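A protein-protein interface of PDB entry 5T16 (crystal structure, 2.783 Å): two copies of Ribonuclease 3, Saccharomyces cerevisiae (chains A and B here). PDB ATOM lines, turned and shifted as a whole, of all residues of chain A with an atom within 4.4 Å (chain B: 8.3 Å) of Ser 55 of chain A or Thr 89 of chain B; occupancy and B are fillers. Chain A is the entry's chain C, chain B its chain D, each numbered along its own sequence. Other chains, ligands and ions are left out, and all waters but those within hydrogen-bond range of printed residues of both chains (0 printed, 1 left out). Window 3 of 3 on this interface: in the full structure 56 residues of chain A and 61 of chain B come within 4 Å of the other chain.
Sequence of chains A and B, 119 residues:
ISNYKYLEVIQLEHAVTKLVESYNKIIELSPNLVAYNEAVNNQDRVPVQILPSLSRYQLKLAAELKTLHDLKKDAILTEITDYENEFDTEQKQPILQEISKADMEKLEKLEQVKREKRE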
ATOM      1  N   LEU A  51      -5.112   5.415  -7.142  1.00  0.00           N
ATOM      2  CA  LEU A  51      -4.363   4.493  -7.989  1.00  0.00           C
ATOM      3  C   LEU A  51      -3.052   4.028  -7.368  1.00  0.00           C
ATOM      4  O   LEU A  51      -2.740   2.845  -7.432  1.00  0.00           O
ATOM      5  CB  LEU A  51      -4.111   5.089  -9.374  1.00  0.00           C
ATOM      6  CG  LEU A  51      -5.168   4.690 -10.390  1.00  0.00           C
ATOM      7  CD1 LEU A  51      -4.856   5.275 -11.713  1.00  0.00           C
ATOM      8  CD2 LEU A  51      -5.151   3.199 -10.512  1.00  0.00           C
ATOM      9  N   PRO A  52      -2.267   4.944  -6.791  1.00  0.00           N
ATOM     10  CA  PRO A  52      -1.058   4.416  -6.158  1.00  0.00           C
ATOM     11  C   PRO A  52      -1.319   3.352  -5.079  1.00  0.00           C
ATOM     12  O   PRO A  52      -0.467   2.488  -4.881  1.00  0.00           O
ATOM     13  CB  PRO A  52      -0.379   5.666  -5.584  1.00  0.00           C
ATOM     14  CG  PRO A  52      -1.311   6.801  -5.843  1.00  0.00           C
ATOM     15  CD  PRO A  52      -2.199   6.404  -6.946  1.00  0.00           C
ATOM     16  N   SER A  53      -2.467   3.383  -4.420  1.00  0.00           N
ATOM     17  CA  SER A  53      -2.756   2.399  -3.374  1.00  0.00           C
ATOM     18  C   SER A  53      -2.684   0.970  -3.900  1.00  0.00           C
ATOM     19  O   SER A  53      -2.434   0.028  -3.144  1.00  0.00           O
ATOM     20  CB  SER A  53      -4.145   2.647  -2.774  1.00  0.00           C
ATOM     21  OG  SER A  53      -4.417   4.041  -2.656  1.00  0.00           O
ATOM     22  N   LEU A  54      -2.933   0.815  -5.195  1.00  0.00           N
ATOM     23  CA  LEU A  54      -2.968  -0.496  -5.832  1.00  0.00           C
ATOM     24  C   LEU A  54      -1.592  -1.090  -6.113  1.00  0.00           C
ATOM     25  O   LEU A  54      -1.453  -2.289  -6.354  1.00  0.00           O
ATOM     26  CB  LEU A  54      -3.748  -0.416  -7.136  1.00  0.00           C
ATOM     27  CG  LEU A  54      -5.202   0.012  -6.965  1.00  0.00           C
ATOM     28  CD1 LEU A  54      -5.887   0.116  -8.320  1.00  0.00           C
ATOM     29  CD2 LEU A  54      -5.931  -0.913  -6.027  1.00  0.00           C
ATOM     30  N   SER A  55      -0.591  -0.230  -6.175  1.00  0.00           N
ATOM     31  CA  SER A  55       0.786  -0.666  -6.338  1.00  0.00           C
ATOM     32  C   SER A  55       1.401  -1.076  -5.014  1.00  0.00           C
ATOM     33  O   SER A  55       2.497  -1.606  -5.002  1.00  0.00           O
ATOM     34  CB  SER A  55       1.620   0.434  -6.990  1.00  0.00           C
ATOM     35  OG  SER A  55       0.884   1.105  -8.010  1.00  0.00           O
ATOM     36  N   ARG A  56       0.720  -0.795  -3.903  1.00  0.00           N
ATOM     37  CA  ARG A  56       1.261  -1.087  -2.574  1.00  0.00           C
ATOM     38  C   ARG A  56       0.471  -2.209  -1.901  1.00  0.00           C
ATOM     39  O   ARG A  56      -0.710  -2.422  -2.201  1.00  0.00           O
ATOM     40  CB  ARG A  56       1.221   0.155  -1.689  1.00  0.00           C
ATOM     41  CG  ARG A  56       1.979   1.324  -2.237  1.00  0.00           C
ATOM     42  CD  ARG A  56       2.029   2.473  -1.255  1.00  0.00           C
ATOM     43  NE  ARG A  56       0.755   3.182  -1.188  1.00  0.00           N
ATOM     44  CZ  ARG A  56       0.484   4.300  -1.858  1.00  0.00           C
ATOM     45  NH1 ARG A  56       1.398   4.826  -2.672  1.00  0.00           N
ATOM     46  NH2 ARG A  56      -0.710   4.881  -1.734  1.00  0.00           N
ATOM     47  N   GLU B  13      -4.860   1.927   4.772  1.00  0.00           N
ATOM     48  CA  GLU B  13      -3.449   1.711   4.553  1.00  0.00           C
ATOM     49  C   GLU B  13      -2.702   1.907   5.847  1.00  0.00           C
ATOM     50  O   GLU B  13      -1.824   1.119   6.205  1.00  0.00           O
ATOM     51  CB  GLU B  13      -2.932   2.669   3.482  1.00  0.00           C
ATOM     52  CG  GLU B  13      -3.302   2.252   2.063  1.00  0.00           C
ATOM     53  CD  GLU B  13      -2.652   3.105   0.998  1.00  0.00           C
ATOM     54  OE1 GLU B  13      -2.788   4.345   1.052  1.00  0.00           O
ATOM     55  OE2 GLU B  13      -1.994   2.529   0.107  1.00  0.00           O
ATOM     56  N   GLU B  86       6.075 -10.505   0.154  1.00  0.00           N
ATOM     57  CA  GLU B  86       5.541 -11.448  -0.829  1.00  0.00           C
ATOM     58  C   GLU B  86       4.535 -10.829  -1.802  1.00  0.00           C
ATOM     59  O   GLU B  86       4.042 -11.477  -2.731  1.00  0.00           O
ATOM     60  CB  GLU B  86       4.874 -12.609  -0.122  1.00  0.00           C
ATOM     61  CG  GLU B  86       4.732 -13.797  -1.001  1.00  0.00           C
ATOM     62  CD  GLU B  86       4.928 -15.028  -0.221  1.00  0.00           C
ATOM     63  OE1 GLU B  86       4.572 -15.009   0.986  1.00  0.00           O
ATOM     64  OE2 GLU B  86       5.519 -15.975  -0.793  1.00  0.00           O
ATOM     65  N   PHE B  87       4.272  -9.550  -1.617  1.00  0.00           N
ATOM     66  CA  PHE B  87       3.308  -8.872  -2.449  1.00  0.00           C
ATOM     67  C   PHE B  87       3.928  -8.595  -3.794  1.00  0.00           C
ATOM     68  O   PHE B  87       5.056  -8.133  -3.870  1.00  0.00           O
ATOM     69  CB  PHE B  87       2.839  -7.564  -1.805  1.00  0.00           C
ATOM     70  CG  PHE B  87       1.929  -6.765  -2.680  1.00  0.00           C
ATOM     71  CD1 PHE B  87       0.635  -7.181  -2.915  1.00  0.00           C
ATOM     72  CD2 PHE B  87       2.373  -5.603  -3.278  1.00  0.00           C
ATOM     73  CE1 PHE B  87      -0.206  -6.451  -3.732  1.00  0.00           C
ATOM     74  CE2 PHE B  87       1.538  -4.861  -4.099  1.00  0.00           C
ATOM     75  CZ  PHE B  87       0.247  -5.289  -4.329  1.00  0.00           C
ATOM     76  N   ASP B  88       3.190  -8.894  -4.852  1.00  0.00           N
ATOM     77  CA  ASP B  88       3.609  -8.527  -6.188  1.00  0.00           C
ATOM     78  C   ASP B  88       2.375  -8.087  -6.951  1.00  0.00           C
ATOM     79  O   ASP B  88       1.342  -8.747  -6.880  1.00  0.00           O
ATOM     80  CB  ASP B  88       4.272  -9.700  -6.898  1.00  0.00           C
ATOM     81  CG  ASP B  88       4.856  -9.315  -8.243  1.00  0.00           C
ATOM     82  OD1 ASP B  88       4.589  -8.203  -8.744  1.00  0.00           O
ATOM     83  OD2 ASP B  88       5.557 -10.150  -8.834  1.00  0.00           O
ATOM     84  N   THR B  89       2.481  -6.983  -7.687  1.00  0.00           N
ATOM     85  CA  THR B  89       1.338  -6.452  -8.422  1.00  0.00           C
ATOM     86  C   THR B  89       0.856  -7.394  -9.525  1.00  0.00           C
ATOM     87  O   THR B  89      -0.307  -7.333  -9.923  1.00  0.00           O
ATOM     88  CB  THR B  89       1.654  -5.102  -9.042  1.00  0.00           C
ATOM     89  OG1 THR B  89       2.986  -5.129  -9.551  1.00  0.00           O
ATOM     90  CG2 THR B  89       1.588  -4.025  -8.002  1.00  0.00           C
ATOM     91  N   GLU B  90       1.734  -8.245 -10.054  1.00  0.00           N
ATOM     92  CA  GLU B  90       1.287  -9.146 -11.119  1.00  0.00           C
ATOM     93  C   GLU B  90       0.936 -10.556 -10.670  1.00  0.00           C
ATOM     94  O   GLU B  90       0.664 -11.429 -11.503  1.00  0.00           O
ATOM     95  CB  GLU B  90       2.302  -9.215 -12.223  1.00  0.00           C
ATOM     96  CG  GLU B  90       2.363  -7.925 -12.940  1.00  0.00           C
ATOM     97  CD  GLU B  90       3.312  -7.988 -14.081  1.00  0.00           C
ATOM     98  OE1 GLU B  90       4.023  -9.016 -14.190  1.00  0.00           O
ATOM     99  OE2 GLU B  90       3.358  -7.002 -14.855  1.00  0.00           O
ATOM    100  N   GLN B  91       0.932 -10.762  -9.355  1.00  0.00           N
ATOM    101  CA  GLN B  91       0.266 -11.909  -8.773  1.00  0.00           C
ATOM    102  C   GLN B  91      -1.094 -11.428  -8.360  1.00  0.00           C
ATOM    103  O   GLN B  91      -1.230 -10.647  -7.423  1.00  0.00           O
ATOM    104  CB  GLN B  91       1.047 -12.460  -7.581  1.00  0.00           C
ATOM    105  CG  GLN B  91       0.376 -13.623  -6.844  1.00  0.00           C
ATOM    106  CD  GLN B  91      -0.155 -14.714  -7.771  1.00  0.00           C
ATOM    107  OE1 GLN B  91      -1.362 -14.775  -8.048  1.00  0.00           O
ATOM    108  NE2 GLN B  91       0.744 -15.554  -8.288  1.00  0.00           N
ATOM    109  N   LYS B  92      -2.110 -11.883  -9.077  1.00  0.00           N
ATOM    110  CA  LYS B  92      -3.456 -11.376  -8.861  1.00  0.00           C
ATOM    111  C   LYS B  92      -4.244 -12.337  -8.001  1.00  0.00           C
ATOM    112  O   LYS B  92      -5.463 -12.207  -7.862  1.00  0.00           O
ATOM    113  CB  LYS B  92      -4.175 -11.088 -10.176  1.00  0.00           C
ATOM    114  CG  LYS B  92      -3.448 -10.132 -11.105  1.00  0.00           C
ATOM    115  CD  LYS B  92      -4.359  -9.769 -12.263  1.00  0.00           C
ATOM    116  CE  LYS B  92      -3.853  -8.572 -13.039  1.00  0.00           C
ATOM    117  NZ  LYS B  92      -3.803  -7.366 -12.166  1.00  0.00           N
ATOM    118  N   GLN B  93      -3.557 -13.303  -7.408  1.00  0.00           N
ATOM    119  CA  GLN B  93      -4.285 -14.224  -6.566  1.00  0.00           C
ATOM    120  C   GLN B  93      -3.849 -14.140  -5.121  1.00  0.00           C
ATOM    121  O   GLN B  93      -2.714 -13.739  -4.832  1.00  0.00           O
ATOM    122  CB  GLN B  93      -4.119 -15.650  -7.071  1.00  0.00           C
ATOM    123  CG  GLN B  93      -4.497 -15.778  -8.491  1.00  0.00           C
ATOM    124  CD  GLN B  93      -4.615 -17.206  -8.887  1.00  0.00           C
ATOM    125  OE1 GLN B  93      -5.465 -17.927  -8.349  1.00  0.00           O
ATOM    126  NE2 GLN B  93      -3.764 -17.648  -9.815  1.00  0.00           N
ATOM    127  N   ILE B  95      -2.629 -14.082  -1.446  1.00  0.00           N
ATOM    128  CA  ILE B  95      -1.354 -14.457  -0.888  1.00  0.00           C
ATOM    129  C   ILE B  95      -1.608 -15.237   0.379  1.00  0.00           C
ATOM    130  O   ILE B  95      -0.725 -15.917   0.896  1.00  0.00           O
ATOM    131  CB  ILE B  95      -0.514 -13.218  -0.615  1.00  0.00           C
ATOM    132  CG1 ILE B  95      -0.421 -12.381  -1.900  1.00  0.00           C
ATOM    133  CG2 ILE B  95       0.851 -13.595  -0.082  1.00  0.00           C
ATOM    134  CD1 ILE B  95       0.607 -11.260  -1.852  1.00  0.00           C
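Of chain B, only Phe 87 and Thr 89 come within 4 Å of Ser 55 of chain A.
Thr 89 of chain B touches just these residues of chain A: Leu 54 and Ser 55.
Of the printed residues of chain B, Arg 56 of chain A touches Glu 13 and Phe 87.
Of the printed residues of chain A, Glu 13 of chain B touches Ser 53 and Arg 56.
Printed residues of chain B within 4 Å of Ser 53 of chain A: Glu 13 (3.6 Å).
Glu 90 of chain B touches none of the printed residues of chain A.
The nearest residue of chain B that does not touch Ser 55 of chain A is Asp 88 of chain B (6.8 Å).
The nearest printed residue of chain A that does not touch Thr 89 of chain B is Arg 56 of chain A (5.3 Å).
Ser 53 of chain A touches Glu 13 of chain B (CA to OE2, 3.6 Å).
O of Leu 54 of chain A touches CZ of Phe 87 of chain B, at 3.999 Å.
Leu 54 of chain A touches Thr 89 of chain B (O to CG2, 3.9 Å).
Ser 55 of chain A touches Phe 87 of chain B (O to CE2, 3.5 Å).
Thr 89 of chain B touches Ser 55 of chain A (CG2 to CA, 3.8 Å).
Phe 87 of chain B touches Arg 56 of chain A.
No position is printed for both chains.
Of the 7 pairs that touch across the chains among the printed residues, none has its exchanged pair printed and touching as well.
Printed residues of chain A that touch a printed residue of chain B: Ser 53, Leu 54, Ser 55 and Arg 56.
Printed residues of chain B that touch a printed residue of chain A: Glu 13, Phe 87 and Thr 89.
Hydrophobic or aromatic side chains of chain B that line the printed part of chain A: Phe 87.
Along chain B the printed residues that touch a printed residue of chain A span positions 13 to 89.
Among the printed residues, 7 pairs touch across the chains.
The guanidinium group (NE) of Arg 56 of chain A lies within salt-bridge range of the side-chain carboxylate (OE2) of Glu 13 of chain B, 3.1 Å away.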
